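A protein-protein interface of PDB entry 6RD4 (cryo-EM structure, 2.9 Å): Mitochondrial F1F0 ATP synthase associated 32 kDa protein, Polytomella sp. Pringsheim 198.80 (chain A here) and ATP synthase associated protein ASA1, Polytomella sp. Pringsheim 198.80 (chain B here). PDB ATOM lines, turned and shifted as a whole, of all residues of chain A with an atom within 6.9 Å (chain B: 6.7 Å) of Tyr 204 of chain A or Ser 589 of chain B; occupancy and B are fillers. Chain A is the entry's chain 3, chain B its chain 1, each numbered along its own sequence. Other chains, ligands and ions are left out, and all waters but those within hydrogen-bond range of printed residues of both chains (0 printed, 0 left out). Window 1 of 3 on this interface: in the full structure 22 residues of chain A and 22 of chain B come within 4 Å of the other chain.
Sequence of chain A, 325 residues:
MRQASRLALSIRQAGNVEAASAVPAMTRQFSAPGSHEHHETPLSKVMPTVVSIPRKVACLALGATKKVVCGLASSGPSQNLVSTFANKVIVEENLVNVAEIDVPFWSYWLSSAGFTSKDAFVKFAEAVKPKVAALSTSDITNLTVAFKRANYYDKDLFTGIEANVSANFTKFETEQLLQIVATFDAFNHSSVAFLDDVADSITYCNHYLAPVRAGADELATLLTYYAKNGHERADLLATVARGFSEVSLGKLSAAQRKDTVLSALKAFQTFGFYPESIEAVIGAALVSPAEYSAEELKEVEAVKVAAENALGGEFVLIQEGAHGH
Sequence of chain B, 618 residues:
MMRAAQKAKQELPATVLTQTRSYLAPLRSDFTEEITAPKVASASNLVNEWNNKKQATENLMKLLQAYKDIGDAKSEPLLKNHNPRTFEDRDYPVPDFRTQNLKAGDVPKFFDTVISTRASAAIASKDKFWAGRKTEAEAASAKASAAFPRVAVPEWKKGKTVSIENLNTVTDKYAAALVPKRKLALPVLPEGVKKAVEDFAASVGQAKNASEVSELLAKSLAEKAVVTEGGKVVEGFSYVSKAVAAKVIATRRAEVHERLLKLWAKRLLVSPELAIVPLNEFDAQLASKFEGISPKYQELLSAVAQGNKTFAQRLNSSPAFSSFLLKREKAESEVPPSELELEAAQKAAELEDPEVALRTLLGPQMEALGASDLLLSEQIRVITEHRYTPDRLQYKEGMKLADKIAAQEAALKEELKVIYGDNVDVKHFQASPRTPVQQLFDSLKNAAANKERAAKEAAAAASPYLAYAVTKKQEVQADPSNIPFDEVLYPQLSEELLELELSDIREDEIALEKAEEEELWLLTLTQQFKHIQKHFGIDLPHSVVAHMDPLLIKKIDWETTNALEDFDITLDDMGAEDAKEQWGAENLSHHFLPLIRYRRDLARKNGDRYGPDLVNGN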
ATOM      1  N   PHE A 169     -25.898  -6.531  23.483  1.00  0.00           N
ATOM      2  CA  PHE A 169     -24.710  -7.178  22.956  1.00  0.00           C
ATOM      3  C   PHE A 169     -23.525  -7.069  23.890  1.00  0.00           C
ATOM      4  O   PHE A 169     -22.609  -7.880  23.798  1.00  0.00           O
ATOM      5  CB  PHE A 169     -24.375  -6.619  21.577  1.00  0.00           C
ATOM      6  CG  PHE A 169     -23.786  -5.246  21.588  1.00  0.00           C
ATOM      7  CD1 PHE A 169     -24.574  -4.139  21.782  1.00  0.00           C
ATOM      8  CD2 PHE A 169     -22.446  -5.062  21.356  1.00  0.00           C
ATOM      9  CE1 PHE A 169     -24.028  -2.897  21.787  1.00  0.00           C
ATOM     10  CE2 PHE A 169     -21.910  -3.830  21.360  1.00  0.00           C
ATOM     11  CZ  PHE A 169     -22.699  -2.748  21.573  1.00  0.00           C
ATOM     12  N   ALA A 199     -20.097  -9.044  16.181  1.00  0.00           N
ATOM     13  CA  ALA A 199     -18.684  -8.760  15.999  1.00  0.00           C
ATOM     14  C   ALA A 199     -18.197  -7.668  16.929  1.00  0.00           C
ATOM     15  O   ALA A 199     -17.015  -7.639  17.269  1.00  0.00           O
ATOM     16  CB  ALA A 199     -18.419  -8.360  14.561  1.00  0.00           C
ATOM     17  N   ASP A 200     -19.069  -6.739  17.322  1.00  0.00           N
ATOM     18  CA  ASP A 200     -18.675  -5.722  18.286  1.00  0.00           C
ATOM     19  C   ASP A 200     -18.524  -6.316  19.663  1.00  0.00           C
ATOM     20  O   ASP A 200     -17.736  -5.824  20.465  1.00  0.00           O
ATOM     21  CB  ASP A 200     -19.697  -4.599  18.347  1.00  0.00           C
ATOM     22  CG  ASP A 200     -19.520  -3.586  17.253  1.00  0.00           C
ATOM     23  OD1 ASP A 200     -18.493  -3.630  16.560  1.00  0.00           O
ATOM     24  OD2 ASP A 200     -20.413  -2.736  17.082  1.00  0.00           O
ATOM     25  N   SER A 201     -19.268  -7.367  19.946  1.00  0.00           N
ATOM     26  CA  SER A 201     -19.276  -7.966  21.259  1.00  0.00           C
ATOM     27  C   SER A 201     -18.141  -8.948  21.444  1.00  0.00           C
ATOM     28  O   SER A 201     -17.588  -9.049  22.531  1.00  0.00           O
ATOM     29  CB  SER A 201     -20.596  -8.664  21.472  1.00  0.00           C
ATOM     30  OG  SER A 201     -20.563  -9.375  22.676  1.00  0.00           O
ATOM     31  N   ILE A 202     -17.788  -9.690  20.406  1.00  0.00           N
ATOM     32  CA  ILE A 202     -16.672 -10.611  20.499  1.00  0.00           C
ATOM     33  C   ILE A 202     -15.364  -9.852  20.559  1.00  0.00           C
ATOM     34  O   ILE A 202     -14.429 -10.257  21.254  1.00  0.00           O
ATOM     35  CB  ILE A 202     -16.746 -11.603  19.326  1.00  0.00           C
ATOM     36  CG1 ILE A 202     -17.871 -12.591  19.572  1.00  0.00           C
ATOM     37  CG2 ILE A 202     -15.483 -12.378  19.134  1.00  0.00           C
ATOM     38  CD1 ILE A 202     -18.092 -13.542  18.473  1.00  0.00           C
ATOM     39  N   THR A 203     -15.294  -8.701  19.907  1.00  0.00           N
ATOM     40  CA  THR A 203     -14.028  -7.996  19.799  1.00  0.00           C
ATOM     41  C   THR A 203     -13.804  -7.049  20.962  1.00  0.00           C
ATOM     42  O   THR A 203     -12.704  -6.985  21.515  1.00  0.00           O
ATOM     43  CB  THR A 203     -13.985  -7.225  18.504  1.00  0.00           C
ATOM     44  OG1 THR A 203     -14.499  -8.046  17.471  1.00  0.00           O
ATOM     45  CG2 THR A 203     -12.589  -6.891  18.181  1.00  0.00           C
ATOM     46  N   TYR A 204     -14.826  -6.290  21.333  1.00  0.00           N
ATOM     47  CA  TYR A 204     -14.686  -5.207  22.286  1.00  0.00           C
ATOM     48  C   TYR A 204     -15.330  -5.484  23.620  1.00  0.00           C
ATOM     49  O   TYR A 204     -14.796  -5.073  24.636  1.00  0.00           O
ATOM     50  CB  TYR A 204     -15.282  -3.922  21.714  1.00  0.00           C
ATOM     51  CG  TYR A 204     -14.674  -3.549  20.413  1.00  0.00           C
ATOM     52  CD1 TYR A 204     -13.450  -2.951  20.368  1.00  0.00           C
ATOM     53  CD2 TYR A 204     -15.319  -3.813  19.229  1.00  0.00           C
ATOM     54  CE1 TYR A 204     -12.879  -2.636  19.193  1.00  0.00           C
ATOM     55  CE2 TYR A 204     -14.752  -3.501  18.045  1.00  0.00           C
ATOM     56  CZ  TYR A 204     -13.531  -2.916  18.034  1.00  0.00           C
ATOM     57  OH  TYR A 204     -12.950  -2.587  16.846  1.00  0.00           O
ATOM     58  N   CYS A 205     -16.454  -6.158  23.653  1.00  0.00           N
ATOM     59  CA  CYS A 205     -17.135  -6.378  24.907  1.00  0.00           C
ATOM     60  C   CYS A 205     -16.695  -7.651  25.596  1.00  0.00           C
ATOM     61  O   CYS A 205     -17.207  -7.957  26.668  1.00  0.00           O
ATOM     62  CB  CYS A 205     -18.637  -6.417  24.676  1.00  0.00           C
ATOM     63  SG  CYS A 205     -19.300  -4.994  23.845  1.00  0.00           S
ATOM     64  N   ASN A 206     -15.781  -8.405  25.012  1.00  0.00           N
ATOM     65  CA  ASN A 206     -15.359  -9.671  25.568  1.00  0.00           C
ATOM     66  C   ASN A 206     -13.854  -9.737  25.621  1.00  0.00           C
ATOM     67  O   ASN A 206     -13.167  -9.041  24.879  1.00  0.00           O
ATOM     68  CB  ASN A 206     -15.887 -10.824  24.763  1.00  0.00           C
ATOM     69  CG  ASN A 206     -17.219 -11.246  25.211  1.00  0.00           C
ATOM     70  OD1 ASN A 206     -18.213 -11.034  24.551  1.00  0.00           O
ATOM     71  ND2 ASN A 206     -17.255 -11.876  26.353  1.00  0.00           N
ATOM     72  N   HIS A 207     -13.356 -10.596  26.508  1.00  0.00           N
ATOM     73  CA  HIS A 207     -11.928 -10.734  26.723  1.00  0.00           C
ATOM     74  C   HIS A 207     -11.246 -11.207  25.458  1.00  0.00           C
ATOM     75  O   HIS A 207     -11.805 -11.982  24.693  1.00  0.00           O
ATOM     76  CB  HIS A 207     -11.655 -11.716  27.842  1.00  0.00           C
ATOM     77  CG  HIS A 207     -10.286 -11.593  28.417  1.00  0.00           C
ATOM     78  ND1 HIS A 207      -9.196 -12.216  27.871  1.00  0.00           N
ATOM     79  CD2 HIS A 207      -9.824 -10.889  29.466  1.00  0.00           C
ATOM     80  CE1 HIS A 207      -8.121 -11.916  28.568  1.00  0.00           C
ATOM     81  NE2 HIS A 207      -8.476 -11.105  29.538  1.00  0.00           N
ATOM     82  N   ARG A 233     -15.405  -7.574   8.705  1.00  0.00           N
ATOM     83  CA  ARG A 233     -15.078  -6.900   9.956  1.00  0.00           C
ATOM     84  C   ARG A 233     -13.649  -7.310  10.232  1.00  0.00           C
ATOM     85  O   ARG A 233     -13.433  -8.381  10.780  1.00  0.00           O
ATOM     86  CB  ARG A 233     -15.996  -7.333  11.074  1.00  0.00           C
ATOM     87  CG  ARG A 233     -17.411  -6.869  10.962  1.00  0.00           C
ATOM     88  CD  ARG A 233     -17.505  -5.422  11.293  1.00  0.00           C
ATOM     89  NE  ARG A 233     -16.729  -5.118  12.475  1.00  0.00           N
ATOM     90  CZ  ARG A 233     -17.251  -4.947  13.673  1.00  0.00           C
ATOM     91  NH1 ARG A 233     -16.473  -4.672  14.698  1.00  0.00           N
ATOM     92  NH2 ARG A 233     -18.552  -5.039  13.835  1.00  0.00           N
ATOM     93  N   ASP A 235     -11.562  -6.266  12.329  1.00  0.00           N
ATOM     94  CA  ASP A 235     -11.240  -6.334  13.744  1.00  0.00           C
ATOM     95  C   ASP A 235     -11.694  -7.648  14.352  1.00  0.00           C
ATOM     96  O   ASP A 235     -11.013  -8.196  15.220  1.00  0.00           O
ATOM     97  CB  ASP A 235     -11.848  -5.133  14.458  1.00  0.00           C
ATOM     98  CG  ASP A 235     -13.308  -4.940  14.147  1.00  0.00           C
ATOM     99  OD1 ASP A 235     -13.884  -5.729  13.399  1.00  0.00           O
ATOM    100  OD2 ASP A 235     -13.894  -3.960  14.623  1.00  0.00           O
ATOM    101  N   LEU A 236     -12.833  -8.173  13.899  1.00  0.00           N
ATOM    102  CA  LEU A 236     -13.297  -9.472  14.363  1.00  0.00           C
ATOM    103  C   LEU A 236     -12.399 -10.583  13.861  1.00  0.00           C
ATOM    104  O   LEU A 236     -12.174 -11.564  14.564  1.00  0.00           O
ATOM    105  CB  LEU A 236     -14.727  -9.712  13.903  1.00  0.00           C
ATOM    106  CG  LEU A 236     -15.341 -11.072  14.198  1.00  0.00           C
ATOM    107  CD1 LEU A 236     -15.771 -11.144  15.606  1.00  0.00           C
ATOM    108  CD2 LEU A 236     -16.497 -11.338  13.312  1.00  0.00           C
ATOM    109  N   THR A 239      -9.428 -11.150  15.978  1.00  0.00           N
ATOM    110  CA  THR A 239      -9.808 -11.736  17.249  1.00  0.00           C
ATOM    111  C   THR A 239     -10.015 -13.233  17.126  1.00  0.00           C
ATOM    112  O   THR A 239      -9.473 -13.998  17.920  1.00  0.00           O
ATOM    113  CB  THR A 239     -11.073 -11.047  17.752  1.00  0.00           C
ATOM    114  OG1 THR A 239     -10.786  -9.678  18.003  1.00  0.00           O
ATOM    115  CG2 THR A 239     -11.544 -11.635  19.000  1.00  0.00           C
ATOM    116  N   LEU B 551     -17.738  -3.279  31.548  1.00  0.00           N
ATOM    117  CA  LEU B 551     -17.079  -4.232  30.684  1.00  0.00           C
ATOM    118  C   LEU B 551     -15.625  -4.416  31.021  1.00  0.00           C
ATOM    119  O   LEU B 551     -15.003  -5.310  30.475  1.00  0.00           O
ATOM    120  CB  LEU B 551     -17.177  -3.801  29.228  1.00  0.00           C
ATOM    121  CG  LEU B 551     -18.516  -3.706  28.538  1.00  0.00           C
ATOM    122  CD1 LEU B 551     -18.291  -3.316  27.136  1.00  0.00           C
ATOM    123  CD2 LEU B 551     -19.168  -5.019  28.575  1.00  0.00           C
ATOM    124  N   LYS B 555     -14.459  -8.291  31.819  1.00  0.00           N
ATOM    125  CA  LYS B 555     -13.287  -8.937  31.257  1.00  0.00           C
ATOM    126  C   LYS B 555     -12.282  -9.340  32.313  1.00  0.00           C
ATOM    127  O   LYS B 555     -11.509 -10.260  32.088  1.00  0.00           O
ATOM    128  CB  LYS B 555     -12.603  -8.013  30.275  1.00  0.00           C
ATOM    129  CG  LYS B 555     -13.382  -7.711  29.073  1.00  0.00           C
ATOM    130  CD  LYS B 555     -12.600  -6.841  28.188  1.00  0.00           C
ATOM    131  CE  LYS B 555     -13.451  -5.833  27.572  1.00  0.00           C
ATOM    132  NZ  LYS B 555     -12.795  -5.304  26.393  1.00  0.00           N
ATOM    133  N   GLY B 584      -3.250  -4.969  28.347  1.00  0.00           N
ATOM    134  CA  GLY B 584      -3.906  -3.811  28.900  1.00  0.00           C
ATOM    135  C   GLY B 584      -4.730  -3.065  27.886  1.00  0.00           C
ATOM    136  O   GLY B 584      -5.780  -2.534  28.218  1.00  0.00           O
ATOM    137  N   ALA B 585      -4.274  -3.007  26.645  1.00  0.00           N
ATOM    138  CA  ALA B 585      -4.993  -2.265  25.629  1.00  0.00           C
ATOM    139  C   ALA B 585      -6.238  -2.983  25.168  1.00  0.00           C
ATOM    140  O   ALA B 585      -7.205  -2.333  24.783  1.00  0.00           O
ATOM    141  CB  ALA B 585      -4.096  -2.010  24.433  1.00  0.00           C
ATOM    142  N   GLU B 586      -6.247  -4.302  25.194  1.00  0.00           N
ATOM    143  CA  GLU B 586      -7.423  -5.053  24.802  1.00  0.00           C
ATOM    144  C   GLU B 586      -8.459  -5.145  25.898  1.00  0.00           C
ATOM    145  O   GLU B 586      -9.547  -5.654  25.648  1.00  0.00           O
ATOM    146  CB  GLU B 586      -7.044  -6.457  24.384  1.00  0.00           C
ATOM    147  CG  GLU B 586      -6.346  -6.535  23.073  1.00  0.00           C
ATOM    148  CD  GLU B 586      -7.272  -6.510  21.902  1.00  0.00           C
ATOM    149  OE1 GLU B 586      -8.451  -6.859  22.068  1.00  0.00           O
ATOM    150  OE2 GLU B 586      -6.818  -6.141  20.805  1.00  0.00           O
ATOM    151  N   ASN B 587      -8.145  -4.716  27.108  1.00  0.00           N
ATOM    152  CA  ASN B 587      -9.099  -4.748  28.194  1.00  0.00           C
ATOM    153  C   ASN B 587      -9.763  -3.419  28.415  1.00  0.00           C
ATOM    154  O   ASN B 587     -10.795  -3.361  29.078  1.00  0.00           O
ATOM    155  CB  ASN B 587      -8.430  -5.168  29.492  1.00  0.00           C
ATOM    156  CG  ASN B 587      -8.326  -6.648  29.634  1.00  0.00           C
ATOM    157  OD1 ASN B 587      -7.705  -7.143  30.550  1.00  0.00           O
ATOM    158  ND2 ASN B 587      -8.933  -7.370  28.724  1.00  0.00           N
ATOM    159  N   LEU B 588      -9.172  -2.356  27.906  1.00  0.00           N
ATOM    160  CA  LEU B 588      -9.818  -1.071  27.772  1.00  0.00           C
ATOM    161  C   LEU B 588     -10.231  -0.823  26.348  1.00  0.00           C
ATOM    162  O   LEU B 588     -10.414   0.321  25.953  1.00  0.00           O
ATOM    163  CB  LEU B 588      -8.881   0.016  28.252  1.00  0.00           C
ATOM    164  CG  LEU B 588      -8.358  -0.276  29.632  1.00  0.00           C
ATOM    165  CD1 LEU B 588      -7.237   0.604  29.840  1.00  0.00           C
ATOM    166  CD2 LEU B 588      -9.424   0.023  30.593  1.00  0.00           C
ATOM    167  N   SER B 589     -10.370  -1.885  25.572  1.00  0.00           N
ATOM    168  CA  SER B 589     -10.634  -1.813  24.150  1.00  0.00           C
ATOM    169  C   SER B 589     -12.012  -1.288  23.854  1.00  0.00           C
ATOM    170  O   SER B 589     -12.241  -0.752  22.776  1.00  0.00           O
ATOM    171  CB  SER B 589     -10.496  -3.202  23.566  1.00  0.00           C
ATOM    172  OG  SER B 589     -10.744  -3.197  22.190  1.00  0.00           O
ATOM    173  N   HIS B 590     -12.917  -1.452  24.784  1.00  0.00           N
ATOM    174  CA  HIS B 590     -14.298  -1.064  24.695  1.00  0.00           C
ATOM    175  C   HIS B 590     -14.512   0.393  25.008  1.00  0.00           C
ATOM    176  O   HIS B 590     -15.652   0.840  25.016  1.00  0.00           O
ATOM    177  CB  HIS B 590     -15.103  -1.891  25.667  1.00  0.00           C
ATOM    178  CG  HIS B 590     -14.616  -1.773  27.071  1.00  0.00           C
ATOM    179  ND1 HIS B 590     -15.178  -0.910  27.974  1.00  0.00           N
ATOM    180  CD2 HIS B 590     -13.597  -2.375  27.717  1.00  0.00           C
ATOM    181  CE1 HIS B 590     -14.534  -0.991  29.117  1.00  0.00           C
ATOM    182  NE2 HIS B 590     -13.573  -1.878  28.987  1.00  0.00           N
ATOM    183  N   HIS B 591     -13.464   1.132  25.336  1.00  0.00           N
ATOM    184  CA  HIS B 591     -13.631   2.553  25.574  1.00  0.00           C
ATOM    185  C   HIS B 591     -13.816   3.293  24.275  1.00  0.00           C
ATOM    186  O   HIS B 591     -14.411   4.366  24.255  1.00  0.00           O
ATOM    187  CB  HIS B 591     -12.437   3.103  26.323  1.00  0.00           C
ATOM    188  CG  HIS B 591     -12.466   2.823  27.785  1.00  0.00           C
ATOM    189  ND1 HIS B 591     -11.558   3.351  28.664  1.00  0.00           N
ATOM    190  CD2 HIS B 591     -13.320   2.093  28.527  1.00  0.00           C
ATOM    191  CE1 HIS B 591     -11.836   2.940  29.881  1.00  0.00           C
ATOM    192  NE2 HIS B 591     -12.903   2.176  29.825  1.00  0.00           N
ATOM    193  N   PHE B 592     -13.321   2.730  23.194  1.00  0.00           N
ATOM    194  CA  PHE B 592     -13.416   3.283  21.864  1.00  0.00           C
ATOM    195  C   PHE B 592     -14.587   2.724  21.100  1.00  0.00           C
ATOM    196  O   PHE B 592     -14.812   3.130  19.969  1.00  0.00           O
ATOM    197  CB  PHE B 592     -12.132   3.003  21.113  1.00  0.00           C
ATOM    198  CG  PHE B 592     -10.926   3.494  21.811  1.00  0.00           C
ATOM    199  CD1 PHE B 592     -10.544   4.800  21.690  1.00  0.00           C
ATOM    200  CD2 PHE B 592     -10.180   2.665  22.596  1.00  0.00           C
ATOM    201  CE1 PHE B 592      -9.456   5.263  22.338  1.00  0.00           C
ATOM    202  CE2 PHE B 592      -9.088   3.141  23.246  1.00  0.00           C
ATOM    203  CZ  PHE B 592      -8.730   4.441  23.101  1.00  0.00           C
ATOM    204  N   LEU B 593     -15.315   1.795  21.689  1.00  0.00           N
ATOM    205  CA  LEU B 593     -16.509   1.256  21.053  1.00  0.00           C
ATOM    206  C   LEU B 593     -17.661   2.247  20.902  1.00  0.00           C
ATOM    207  O   LEU B 593     -18.346   2.168  19.871  1.00  0.00           O
ATOM    208  CB  LEU B 593     -16.971   0.011  21.808  1.00  0.00           C
ATOM    209  CG  LEU B 593     -18.158  -0.732  21.236  1.00  0.00           C
ATOM    210  CD1 LEU B 593     -17.809  -1.178  19.868  1.00  0.00           C
ATOM    211  CD2 LEU B 593     -18.496  -1.878  22.084  1.00  0.00           C
ATOM    212  N   ILE B 596     -16.558   4.087  17.592  1.00  0.00           N
ATOM    213  CA  ILE B 596     -16.553   3.381  16.323  1.00  0.00           C
ATOM    214  C   ILE B 596     -17.857   2.675  16.042  1.00  0.00           C
ATOM    215  O   ILE B 596     -18.005   2.089  14.976  1.00  0.00           O
ATOM    216  CB  ILE B 596     -15.372   2.402  16.261  1.00  0.00           C
ATOM    217  CG1 ILE B 596     -15.620   1.194  17.127  1.00  0.00           C
ATOM    218  CG2 ILE B 596     -14.109   3.116  16.685  1.00  0.00           C
ATOM    219  CD1 ILE B 596     -14.421   0.366  17.297  1.00  0.00           C
ATOM    220  N   ARG B 600     -19.293   4.314  12.487  1.00  0.00           N
ATOM    221  CA  ARG B 600     -19.772   3.321  11.545  1.00  0.00           C
ATOM    222  C   ARG B 600     -21.213   3.576  11.150  1.00  0.00           C
ATOM    223  O   ARG B 600     -21.595   3.290  10.018  1.00  0.00           O
ATOM    224  CB  ARG B 600     -19.622   1.930  12.145  1.00  0.00           C
ATOM    225  CG  ARG B 600     -19.933   0.790  11.232  1.00  0.00           C
ATOM    226  CD  ARG B 600     -20.062  -0.480  12.009  1.00  0.00           C
ATOM    227  NE  ARG B 600     -18.850  -0.781  12.747  1.00  0.00           N
ATOM    228  CZ  ARG B 600     -18.830  -1.294  13.968  1.00  0.00           C
ATOM    229  NH1 ARG B 600     -19.958  -1.563  14.599  1.00  0.00           N
ATOM    230  NH2 ARG B 600     -17.676  -1.538  14.559  1.00  0.00           N
ATOM    231  N   PRO B 612     -11.802   1.446   9.359  1.00  0.00           N
ATOM    232  CA  PRO B 612     -11.086   0.384  10.078  1.00  0.00           C
ATOM    233  C   PRO B 612     -11.801  -0.956  10.142  1.00  0.00           C
ATOM    234  O   PRO B 612     -11.214  -1.912  10.658  1.00  0.00           O
ATOM    235  CB  PRO B 612     -10.910   0.975  11.474  1.00  0.00           C
ATOM    236  CG  PRO B 612     -10.983   2.412  11.276  1.00  0.00           C
ATOM    237  CD  PRO B 612     -11.980   2.625  10.219  1.00  0.00           C
ATOM    238  N   ASP B 613     -13.034  -1.074   9.654  1.00  0.00           N
ATOM    239  CA  ASP B 613     -13.657  -2.385   9.574  1.00  0.00           C
ATOM    240  C   ASP B 613     -13.069  -3.231   8.462  1.00  0.00           C
ATOM    241  O   ASP B 613     -13.216  -4.452   8.493  1.00  0.00           O
ATOM    242  CB  ASP B 613     -15.158  -2.260   9.335  1.00  0.00           C
ATOM    243  CG  ASP B 613     -15.921  -1.895  10.577  1.00  0.00           C
ATOM    244  OD1 ASP B 613     -15.299  -1.741  11.639  1.00  0.00           O
ATOM    245  OD2 ASP B 613     -17.155  -1.760  10.490  1.00  0.00           O
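OD1 of Asp 613 of chain B is in salt-bridge range of NE of Arg 233 of chain A (3.8 Å). NH1 of Arg 233 of chain A lies close to NH2 of Arg 600 of chain B (3.4 Å). OD2 of Asp 200 of chain A lies within salt-bridge range of NH1 of Arg 600 of chain B, at 2.8 Å. NZ of Lys 555 of chain B sits at hydrogen-bond distance from O of Tyr 204 of chain A (2.7 Å).
Of the printed residues of chain B, Asp 200 of chain A touches Leu 593 (3.9 Å) and Arg 600 (2.8 Å). Tyr 204 of chain A touches just these residues of chain B: Lys 555, Ser 589, His 590, Leu 593 and Ile 596. Of the printed residues of chain B, Cys 205 of chain A touches Leu 551 and Leu 593. Leu 236 of chain A touches none of the printed residues of chain B. Printed residues of chain A within 4 Å of Leu 551 of chain B: Cys 205 (3.8 Å). Of chain A, only Tyr 204 comes within 4 Å of Ser 589 of chain B. Pro 612 of chain B touches none of the printed residues of chain A. The nearest printed residue of chain A that does not touch Leu 551 of chain B is Tyr 204 of chain A (4.6 Å).
The backbone carbonyl oxygen (O) of Asn 587 of chain B lies within hydrogen-bond range of a ring nitrogen (NE2) of His 590 of chain B, at 3.2 Å. The side-chain hydroxyl (OG) of Ser 201 of chain A is in hydrogen-bond range of the backbone carbonyl oxygen (O) of Phe 169 of chain A. The side-chain amino group (NZ) of Lys 555 of chain B sits at hydrogen-bond distance from the backbone carbonyl oxygen (O) of Glu 586 of chain B (3.4 Å). OH of Tyr 204 of chain A sits at hydrogen-bond distance from OD2 of Asp 235 of chain A (2.8 Å). The backbone carbonyl oxygen (O) of Asp 235 of chain A lies within hydrogen-bond range of the side-chain hydroxyl (OG1) of Thr 239 of chain A, at 3.2 Å. The backbone carbonyl oxygen (O) of Asp 200 of chain A sits at hydrogen-bond distance from the backbone NH (N) of Cys 205 of chain A (3.5 Å).
Printed residues of chain B that touch a printed residue of chain A: Leu 551, Lys 555, Asn 587, Ser 589, His 590, Leu 593, Ile 596, Arg 600 and Asp 613. Hydrophobic or aromatic side chains of chain B within 4 Å of the printed part of chain A: Leu 551, His 590, Leu 593 and Ile 596. Of the 14 printed residues of chain A, 7 touch a printed residue of chain B. Printed residues of chain A that touch a printed residue of chain B: Phe 169, Asp 200, Tyr 204, Cys 205, His 207, Arg 233 and Asp 235. Hydrophobic or aromatic side chains of chain A within 4 Å of the printed part of chain B: Phe 169, Tyr 204 and His 207. Along chain A the printed residues that touch a printed residue of chain B span positions 169 to 235.
Among the printed residues, merely in contact across the chains: His 207 of chain A with Lys 555 of chain B (3.2 Å), Tyr 204 of chain A with Ser 589 of chain B (3.3 Å), Tyr 204 of chain A with Ile 596 of chain B (3.3 Å), Tyr 204 of chain A with His 590 of chain B (3.4 Å), Cys 205 of chain A with Leu 593 of chain B (3.7 Å), Tyr 204 of chain A with Leu 593 of chain B (3.7 Å), His 207 of chain A with Asn 587 of chain B (3.7 Å), Cys 205 of chain A with Leu 551 of chain B (3.8 Å), Asp 200 of chain A with Leu 593 of chain B (3.9 Å), Asp 235 of chain A with Asp 613 of chain B (3.98 Å) and Phe 169 of chain A with Leu 593 of chain B (3.999 Å).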
